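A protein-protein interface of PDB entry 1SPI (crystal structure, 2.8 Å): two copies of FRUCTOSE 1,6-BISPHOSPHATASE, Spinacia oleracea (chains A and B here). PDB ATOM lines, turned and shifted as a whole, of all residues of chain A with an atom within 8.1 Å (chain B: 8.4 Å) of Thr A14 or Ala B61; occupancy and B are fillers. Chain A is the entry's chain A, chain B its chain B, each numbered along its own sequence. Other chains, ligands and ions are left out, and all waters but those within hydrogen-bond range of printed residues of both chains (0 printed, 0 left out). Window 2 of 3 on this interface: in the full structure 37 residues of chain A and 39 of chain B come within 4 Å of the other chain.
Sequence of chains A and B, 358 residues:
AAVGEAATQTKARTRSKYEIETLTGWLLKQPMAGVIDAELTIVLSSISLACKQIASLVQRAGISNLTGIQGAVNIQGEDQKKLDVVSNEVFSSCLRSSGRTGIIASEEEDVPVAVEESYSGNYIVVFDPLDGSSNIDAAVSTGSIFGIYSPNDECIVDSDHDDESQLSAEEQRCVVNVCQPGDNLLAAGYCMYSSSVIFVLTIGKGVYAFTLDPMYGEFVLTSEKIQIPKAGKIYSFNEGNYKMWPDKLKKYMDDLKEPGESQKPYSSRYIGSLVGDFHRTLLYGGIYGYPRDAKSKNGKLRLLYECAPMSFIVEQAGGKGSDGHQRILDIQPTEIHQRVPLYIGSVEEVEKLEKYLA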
ATOM      1  N   THR A  10     -26.543  -0.651 -20.120  1.00  0.00           N
ATOM      2  CA  THR A  10     -25.511   0.256 -19.638  1.00  0.00           C
ATOM      3  C   THR A  10     -24.740  -0.449 -18.563  1.00  0.00           C
ATOM      4  O   THR A  10     -25.002  -1.625 -18.245  1.00  0.00           O
ATOM      5  CB  THR A  10     -25.941   1.661 -19.009  1.00  0.00           C
ATOM      6  OG1 THR A  10     -26.598   1.474 -17.748  1.00  0.00           O
ATOM      7  CG2 THR A  10     -26.694   2.571 -19.958  1.00  0.00           C
ATOM      8  N   LYS A  11     -24.005   0.433 -17.856  1.00  0.00           N
ATOM      9  CA  LYS A  11     -23.065   0.140 -16.778  1.00  0.00           C
ATOM     10  C   LYS A  11     -23.645  -0.486 -15.410  1.00  0.00           C
ATOM     11  O   LYS A  11     -23.028  -0.492 -14.410  1.00  0.00           O
ATOM     12  CB  LYS A  11     -21.919   1.322 -16.639  1.00  0.00           C
ATOM     13  CG  LYS A  11     -20.903   1.918 -17.836  1.00  0.00           C
ATOM     14  CD  LYS A  11     -19.258   1.756 -17.700  1.00  0.00           C
ATOM     15  CE  LYS A  11     -18.302   3.096 -18.352  1.00  0.00           C
ATOM     16  NZ  LYS A  11     -17.733   4.457 -17.923  1.00  0.00           N
ATOM     17  N   ALA A  12     -24.833  -1.130 -15.438  1.00  0.00           N
ATOM     18  CA  ALA A  12     -25.270  -1.774 -14.188  1.00  0.00           C
ATOM     19  C   ALA A  12     -24.293  -2.918 -13.911  1.00  0.00           C
ATOM     20  O   ALA A  12     -23.611  -2.948 -12.872  1.00  0.00           O
ATOM     21  CB  ALA A  12     -26.663  -2.316 -14.292  1.00  0.00           C
ATOM     22  N   ARG A  13     -24.008  -3.731 -14.919  1.00  0.00           N
ATOM     23  CA  ARG A  13     -23.085  -4.858 -14.729  1.00  0.00           C
ATOM     24  C   ARG A  13     -23.584  -5.815 -13.623  1.00  0.00           C
ATOM     25  O   ARG A  13     -22.866  -6.726 -13.182  1.00  0.00           O
ATOM     26  CB  ARG A  13     -21.638  -4.358 -14.503  1.00  0.00           C
ATOM     27  CG  ARG A  13     -20.975  -3.662 -15.731  1.00  0.00           C
ATOM     28  CD  ARG A  13     -20.842  -4.595 -16.975  1.00  0.00           C
ATOM     29  NE  ARG A  13     -19.770  -4.131 -17.861  1.00  0.00           N
ATOM     30  CZ  ARG A  13     -19.582  -4.508 -19.126  1.00  0.00           C
ATOM     31  NH1 ARG A  13     -20.382  -5.369 -19.725  1.00  0.00           N
ATOM     32  NH2 ARG A  13     -18.555  -4.027 -19.798  1.00  0.00           N
ATOM     33  N   THR A  14     -24.817  -5.568 -13.184  1.00  0.00           N
ATOM     34  CA  THR A  14     -25.503  -6.425 -12.217  1.00  0.00           C
ATOM     35  C   THR A  14     -27.001  -6.413 -12.577  1.00  0.00           C
ATOM     36  O   THR A  14     -27.455  -7.212 -13.402  1.00  0.00           O
ATOM     37  CB  THR A  14     -25.269  -6.003 -10.737  1.00  0.00           C
ATOM     38  OG1 THR A  14     -25.358  -4.571 -10.594  1.00  0.00           O
ATOM     39  CG2 THR A  14     -23.902  -6.529 -10.253  1.00  0.00           C
ATOM     40  N   ARG A  15     -27.716  -5.390 -12.116  1.00  0.00           N
ATOM     41  CA  ARG A  15     -29.143  -5.276 -12.408  1.00  0.00           C
ATOM     42  C   ARG A  15     -29.372  -5.362 -13.909  1.00  0.00           C
ATOM     43  O   ARG A  15     -29.102  -4.401 -14.632  1.00  0.00           O
ATOM     44  CB  ARG A  15     -29.725  -3.954 -11.887  1.00  0.00           C
ATOM     45  CG  ARG A  15     -30.136  -4.002 -10.413  1.00  0.00           C
ATOM     46  CD  ARG A  15     -30.451  -2.613  -9.844  1.00  0.00           C
ATOM     47  NE  ARG A  15     -31.458  -1.943 -10.663  1.00  0.00           N
ATOM     48  CZ  ARG A  15     -32.617  -2.500 -11.032  1.00  0.00           C
ATOM     49  NH1 ARG A  15     -32.950  -3.749 -10.645  1.00  0.00           N
ATOM     50  NH2 ARG A  15     -33.424  -1.826 -11.845  1.00  0.00           N
ATOM     51  N   SER A  16     -29.673  -6.575 -14.370  1.00  0.00           N
ATOM     52  CA  SER A  16     -30.003  -6.792 -15.770  1.00  0.00           C
ATOM     53  C   SER A  16     -30.885  -8.025 -15.811  1.00  0.00           C
ATOM     54  O   SER A  16     -30.688  -8.916 -16.637  1.00  0.00           O
ATOM     55  CB  SER A  16     -28.752  -6.971 -16.647  1.00  0.00           C
ATOM     56  OG  SER A  16     -28.020  -8.156 -16.330  1.00  0.00           O
ATOM     57  N   LYS A  17     -31.902  -8.041 -14.945  1.00  0.00           N
ATOM     58  CA  LYS A  17     -32.850  -9.170 -14.859  1.00  0.00           C
ATOM     59  C   LYS A  17     -33.969  -9.150 -15.938  1.00  0.00           C
ATOM     60  O   LYS A  17     -35.129  -9.516 -15.673  1.00  0.00           O
ATOM     61  CB  LYS A  17     -33.467  -9.227 -13.453  1.00  0.00           C
ATOM     62  CG  LYS A  17     -32.452  -9.447 -12.310  1.00  0.00           C
ATOM     63  CD  LYS A  17     -31.405  -8.348 -12.243  1.00  0.00           C
ATOM     64  CE  LYS A  17     -31.983  -7.024 -11.718  1.00  0.00           C
ATOM     65  NZ  LYS A  17     -33.127  -6.396 -12.472  1.00  0.00           N
ATOM     66  N   TYR A  18     -33.580  -8.766 -17.161  1.00  0.00           N
ATOM     67  CA  TYR A  18     -34.461  -8.661 -18.336  1.00  0.00           C
ATOM     68  C   TYR A  18     -35.431  -9.854 -18.451  1.00  0.00           C
ATOM     69  O   TYR A  18     -36.597  -9.687 -18.830  1.00  0.00           O
ATOM     70  CB  TYR A  18     -33.613  -8.607 -19.616  1.00  0.00           C
ATOM     71  CG  TYR A  18     -32.759  -9.857 -19.787  1.00  0.00           C
ATOM     72  CD1 TYR A  18     -31.754 -10.158 -18.860  1.00  0.00           C
ATOM     73  CD2 TYR A  18     -33.017 -10.791 -20.818  1.00  0.00           C
ATOM     74  CE1 TYR A  18     -31.045 -11.328 -18.932  1.00  0.00           C
ATOM     75  CE2 TYR A  18     -32.308 -11.963 -20.907  1.00  0.00           C
ATOM     76  CZ  TYR A  18     -31.314 -12.228 -19.950  1.00  0.00           C
ATOM     77  OH  TYR A  18     -30.548 -13.384 -19.990  1.00  0.00           O
ATOM     78  N   SER A 196     -23.920 -18.490  -1.672  1.00  0.00           N
ATOM     79  CA  SER A 196     -25.136 -18.185  -2.375  1.00  0.00           C
ATOM     80  C   SER A 196     -26.046 -19.156  -1.671  1.00  0.00           C
ATOM     81  O   SER A 196     -25.644 -19.818  -0.707  1.00  0.00           O
ATOM     82  CB  SER A 196     -25.032 -18.576  -3.847  1.00  0.00           C
ATOM     83  OG  SER A 196     -24.022 -17.827  -4.493  1.00  0.00           O
ATOM     84  N   THR A 211     -30.535 -19.502  -7.830  1.00  0.00           N
ATOM     85  CA  THR A 211     -29.712 -18.696  -6.913  1.00  0.00           C
ATOM     86  C   THR A 211     -30.681 -17.773  -6.207  1.00  0.00           C
ATOM     87  O   THR A 211     -31.681 -17.386  -6.801  1.00  0.00           O
ATOM     88  CB  THR A 211     -28.761 -17.778  -7.682  1.00  0.00           C
ATOM     89  OG1 THR A 211     -27.814 -18.550  -8.422  1.00  0.00           O
ATOM     90  CG2 THR A 211     -28.042 -16.843  -6.751  1.00  0.00           C
ATOM     91  N   LEU A 212     -30.395 -17.392  -4.965  1.00  0.00           N
ATOM     92  CA  LEU A 212     -31.281 -16.506  -4.204  1.00  0.00           C
ATOM     93  C   LEU A 212     -30.867 -15.070  -4.353  1.00  0.00           C
ATOM     94  O   LEU A 212     -30.093 -14.572  -3.524  1.00  0.00           O
ATOM     95  CB  LEU A 212     -31.295 -16.863  -2.706  1.00  0.00           C
ATOM     96  CG  LEU A 212     -32.462 -16.531  -1.779  1.00  0.00           C
ATOM     97  CD1 LEU A 212     -32.018 -16.614  -0.323  1.00  0.00           C
ATOM     98  CD2 LEU A 212     -32.996 -15.167  -2.071  1.00  0.00           C
ATOM     99  N   ASP A 213     -31.367 -14.417  -5.409  1.00  0.00           N
ATOM    100  CA  ASP A 213     -31.123 -12.979  -5.672  1.00  0.00           C
ATOM    101  C   ASP A 213     -31.419 -12.317  -4.319  1.00  0.00           C
ATOM    102  O   ASP A 213     -32.577 -12.162  -3.974  1.00  0.00           O
ATOM    103  CB  ASP A 213     -32.144 -12.492  -6.700  1.00  0.00           C
ATOM    104  CG  ASP A 213     -31.973 -11.052  -7.056  1.00  0.00           C
ATOM    105  OD1 ASP A 213     -31.881 -10.210  -6.159  1.00  0.00           O
ATOM    106  OD2 ASP A 213     -31.917 -10.751  -8.250  1.00  0.00           O
ATOM    107  N   PRO A 214     -30.384 -11.952  -3.531  1.00  0.00           N
ATOM    108  CA  PRO A 214     -30.445 -11.332  -2.203  1.00  0.00           C
ATOM    109  C   PRO A 214     -31.381 -10.123  -1.991  1.00  0.00           C
ATOM    110  O   PRO A 214     -32.181 -10.127  -1.027  1.00  0.00           O
ATOM    111  CB  PRO A 214     -28.977 -10.981  -1.934  1.00  0.00           C
ATOM    112  CG  PRO A 214     -28.452 -10.706  -3.290  1.00  0.00           C
ATOM    113  CD  PRO A 214     -29.000 -11.888  -4.026  1.00  0.00           C
ATOM    114  N   MET A 215     -31.278  -9.094  -2.852  1.00  0.00           N
ATOM    115  CA  MET A 215     -32.115  -7.892  -2.747  1.00  0.00           C
ATOM    116  C   MET A 215     -33.577  -8.284  -2.730  1.00  0.00           C
ATOM    117  O   MET A 215     -34.124  -8.505  -1.652  1.00  0.00           O
ATOM    118  CB  MET A 215     -31.834  -6.913  -3.903  1.00  0.00           C
ATOM    119  CG  MET A 215     -30.483  -6.169  -3.795  1.00  0.00           C
ATOM    120  SD  MET A 215     -30.334  -4.537  -4.661  1.00  0.00           S
ATOM    121  CE  MET A 215     -28.926  -4.946  -5.898  1.00  0.00           C
ATOM    122  N   TYR A 216     -34.161  -8.534  -3.906  1.00  0.00           N
ATOM    123  CA  TYR A 216     -35.589  -8.882  -3.957  1.00  0.00           C
ATOM    124  C   TYR A 216     -35.992 -10.220  -3.368  1.00  0.00           C
ATOM    125  O   TYR A 216     -37.065 -10.717  -3.714  1.00  0.00           O
ATOM    126  CB  TYR A 216     -36.179  -8.807  -5.369  1.00  0.00           C
ATOM    127  CG  TYR A 216     -35.977  -7.488  -6.074  1.00  0.00           C
ATOM    128  CD1 TYR A 216     -35.950  -6.291  -5.369  1.00  0.00           C
ATOM    129  CD2 TYR A 216     -35.711  -7.456  -7.426  1.00  0.00           C
ATOM    130  CE1 TYR A 216     -35.641  -5.098  -6.004  1.00  0.00           C
ATOM    131  CE2 TYR A 216     -35.411  -6.285  -8.054  1.00  0.00           C
ATOM    132  CZ  TYR A 216     -35.370  -5.111  -7.344  1.00  0.00           C
ATOM    133  OH  TYR A 216     -35.006  -3.963  -7.978  1.00  0.00           O
ATOM    134  N   VAL A 220     -34.050 -16.781  -8.332  1.00  0.00           N
ATOM    135  CA  VAL A 220     -34.106 -16.777  -9.808  1.00  0.00           C
ATOM    136  C   VAL A 220     -33.581 -18.088 -10.406  1.00  0.00           C
ATOM    137  O   VAL A 220     -32.743 -18.737  -9.791  1.00  0.00           O
ATOM    138  CB  VAL A 220     -33.280 -15.662 -10.401  1.00  0.00           C
ATOM    139  CG1 VAL A 220     -33.388 -15.677 -11.911  1.00  0.00           C
ATOM    140  CG2 VAL A 220     -33.717 -14.362  -9.818  1.00  0.00           C
ATOM    141  N   GLN B  53     -19.919  -4.418  -0.128  1.00  0.00           N
ATOM    142  CA  GLN B  53     -20.310  -4.293  -1.537  1.00  0.00           C
ATOM    143  C   GLN B  53     -20.010  -5.607  -2.247  1.00  0.00           C
ATOM    144  O   GLN B  53     -20.922  -6.303  -2.662  1.00  0.00           O
ATOM    145  CB  GLN B  53     -19.493  -3.206  -2.247  1.00  0.00           C
ATOM    146  CG  GLN B  53     -19.614  -1.802  -1.693  1.00  0.00           C
ATOM    147  CD  GLN B  53     -20.739  -1.075  -2.340  1.00  0.00           C
ATOM    148  OE1 GLN B  53     -21.659  -0.567  -1.663  1.00  0.00           O
ATOM    149  NE2 GLN B  53     -20.715  -1.049  -3.678  1.00  0.00           N
ATOM    150  N   ALA B  55     -19.383  -8.275  -1.146  1.00  0.00           N
ATOM    151  CA  ALA B  55     -20.081  -9.361  -0.473  1.00  0.00           C
ATOM    152  C   ALA B  55     -21.397  -9.653  -1.166  1.00  0.00           C
ATOM    153  O   ALA B  55     -21.662 -10.796  -1.476  1.00  0.00           O
ATOM    154  CB  ALA B  55     -20.314  -9.041   0.976  1.00  0.00           C
ATOM    155  N   SER B  56     -22.255  -8.664  -1.396  1.00  0.00           N
ATOM    156  CA  SER B  56     -23.474  -9.008  -2.113  1.00  0.00           C
ATOM    157  C   SER B  56     -23.275  -9.156  -3.621  1.00  0.00           C
ATOM    158  O   SER B  56     -24.200  -9.514  -4.371  1.00  0.00           O
ATOM    159  CB  SER B  56     -24.645  -8.108  -1.748  1.00  0.00           C
ATOM    160  OG  SER B  56     -25.517  -8.812  -0.849  1.00  0.00           O
ATOM    161  N   LEU B  57     -22.049  -8.898  -4.058  1.00  0.00           N
ATOM    162  CA  LEU B  57     -21.648  -9.086  -5.457  1.00  0.00           C
ATOM    163  C   LEU B  57     -21.180 -10.575  -5.545  1.00  0.00           C
ATOM    164  O   LEU B  57     -21.345 -11.220  -6.591  1.00  0.00           O
ATOM    165  CB  LEU B  57     -20.494  -8.128  -5.781  1.00  0.00           C
ATOM    166  CG  LEU B  57     -19.786  -7.978  -7.118  1.00  0.00           C
ATOM    167  CD1 LEU B  57     -20.737  -7.691  -8.249  1.00  0.00           C
ATOM    168  CD2 LEU B  57     -18.895  -6.842  -6.923  1.00  0.00           C
ATOM    169  N   VAL B  58     -20.562 -11.086  -4.463  1.00  0.00           N
ATOM    170  CA  VAL B  58     -20.120 -12.466  -4.417  1.00  0.00           C
ATOM    171  C   VAL B  58     -21.366 -13.244  -4.150  1.00  0.00           C
ATOM    172  O   VAL B  58     -21.492 -14.370  -4.607  1.00  0.00           O
ATOM    173  CB  VAL B  58     -19.101 -12.769  -3.310  1.00  0.00           C
ATOM    174  CG1 VAL B  58     -19.468 -13.988  -2.564  1.00  0.00           C
ATOM    175  CG2 VAL B  58     -17.774 -13.024  -3.904  1.00  0.00           C
ATOM    176  N   GLN B  59     -22.329 -12.640  -3.457  1.00  0.00           N
ATOM    177  CA  GLN B  59     -23.565 -13.354  -3.136  1.00  0.00           C
ATOM    178  C   GLN B  59     -24.400 -13.525  -4.339  1.00  0.00           C
ATOM    179  O   GLN B  59     -25.444 -14.147  -4.270  1.00  0.00           O
ATOM    180  CB  GLN B  59     -24.374 -12.640  -2.077  1.00  0.00           C
ATOM    181  CG  GLN B  59     -24.169 -13.202  -0.715  1.00  0.00           C
ATOM    182  CD  GLN B  59     -24.222 -12.122   0.316  1.00  0.00           C
ATOM    183  OE1 GLN B  59     -23.503 -11.129   0.220  1.00  0.00           O
ATOM    184  NE2 GLN B  59     -25.098 -12.283   1.291  1.00  0.00           N
ATOM    185  N   ARG B  60     -23.908 -12.987  -5.450  1.00  0.00           N
ATOM    186  CA  ARG B  60     -24.597 -13.064  -6.730  1.00  0.00           C
ATOM    187  C   ARG B  60     -25.794 -12.149  -6.577  1.00  0.00           C
ATOM    188  O   ARG B  60     -26.388 -12.098  -5.510  1.00  0.00           O
ATOM    189  CB  ARG B  60     -24.978 -14.524  -7.066  1.00  0.00           C
ATOM    190  CG  ARG B  60     -23.942 -15.293  -7.968  1.00  0.00           C
ATOM    191  CD  ARG B  60     -22.594 -15.726  -7.295  1.00  0.00           C
ATOM    192  NE  ARG B  60     -21.512 -15.941  -8.299  1.00  0.00           N
ATOM    193  CZ  ARG B  60     -20.207 -16.214  -8.031  1.00  0.00           C
ATOM    194  NH1 ARG B  60     -19.747 -16.336  -6.775  1.00  0.00           N
ATOM    195  NH2 ARG B  60     -19.315 -16.278  -9.023  1.00  0.00           N
ATOM    196  N   ALA B  61     -26.049 -11.318  -7.575  1.00  0.00           N
ATOM    197  CA  ALA B  61     -27.143 -10.374  -7.476  1.00  0.00           C
ATOM    198  C   ALA B  61     -26.994  -9.420  -8.609  1.00  0.00           C
ATOM    199  O   ALA B  61     -25.828  -9.001  -8.851  1.00  0.00           O
ATOM    200  CB  ALA B  61     -27.075  -9.596  -6.165  1.00  0.00           C
ATOM    201  N   LYS B  82     -17.261 -11.395 -14.968  1.00  0.00           N
ATOM    202  CA  LYS B  82     -16.397 -10.268 -14.485  1.00  0.00           C
ATOM    203  C   LYS B  82     -16.671 -10.030 -13.015  1.00  0.00           C
ATOM    204  O   LYS B  82     -17.805  -9.771 -12.634  1.00  0.00           O
ATOM    205  CB  LYS B  82     -16.670  -9.006 -15.309  1.00  0.00           C
ATOM    206  CG  LYS B  82     -16.257  -9.154 -16.783  1.00  0.00           C
ATOM    207  CD  LYS B  82     -16.545  -7.889 -17.589  1.00  0.00           C
ATOM    208  CE  LYS B  82     -15.439  -7.640 -18.620  1.00  0.00           C
ATOM    209  NZ  LYS B  82     -15.203  -8.813 -19.527  1.00  0.00           N
ATOM    210  N   VAL B  86     -13.998  -6.285 -10.555  1.00  0.00           N
ATOM    211  CA  VAL B  86     -15.102  -5.441 -10.085  1.00  0.00           C
ATOM    212  C   VAL B  86     -14.840  -5.162  -8.623  1.00  0.00           C
ATOM    213  O   VAL B  86     -14.887  -4.009  -8.201  1.00  0.00           O
ATOM    214  CB  VAL B  86     -16.463  -6.096 -10.221  1.00  0.00           C
ATOM    215  CG1 VAL B  86     -17.507  -5.177  -9.722  1.00  0.00           C
ATOM    216  CG2 VAL B  86     -16.753  -6.403 -11.646  1.00  0.00           C
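OG1 of Thr A14 sits at hydrogen-bond distance from O of Ala A12. The side-chain hydroxyl (OG) of Ser A16 is in hydrogen-bond range of the backbone carbonyl oxygen (O) of Thr A14 (3.1 Å). N of Val A220 is in hydrogen-bond range of O of Thr A211 (2.9 Å). The side-chain amide oxygen of Gln B59 lies close to the backbone carbonyl oxygen of Ala B55. OE1 of Gln B59 lies close to N of Ser B56. The backbone carbonyl oxygen of Val B58 lies close to the guanidinium group of Arg B60.
Among the printed residues, pairs that only touch across the chains: Pro A214 with Arg B60, Pro A214 with Ala B61, Thr A14 with Ala B61, Ser A196 with Arg B60, Thr A211 with Arg B60, Thr A14 with Leu B57 and Ser A196 with Gln B59.
Thr A14 touches two residues of chain B. Printed residues of chain B within 4 Å of Ser A196: Gln B59 (3.95 Å) and Arg B60 (3.8 Å). Of the printed residues of chain B, Pro A214 touches Arg B60 (3.0 Å) and Ala B61 (3.4 Å). Of the printed residues of chain A, Gln B59 touches Ser A196 (3.95 Å). Printed residues of chain A within 4 Å of Arg B60: Ser A196 (3.8 Å), Thr A211 (3.9 Å) and Pro A214 (3.0 Å). The nearest residue of chain B that does not touch Thr A14 is Val B86 (6.6 Å). The nearest printed residue of chain A that does not touch Arg B60 is Asp A213 (4.8 Å).
Of the 10 printed residues of chain B, 4 touch a printed residue of chain A. Hydrophobic or aromatic side chains of chain B within 4 Å of the printed part of chain A: Leu B57 and Ala B61. Hydrophobic or aromatic side chains of chain A within 4 Å of the printed part of chain B: Pro A214. Among the printed residues, 7 pairs touch across the chains.
No position is printed for both chains.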
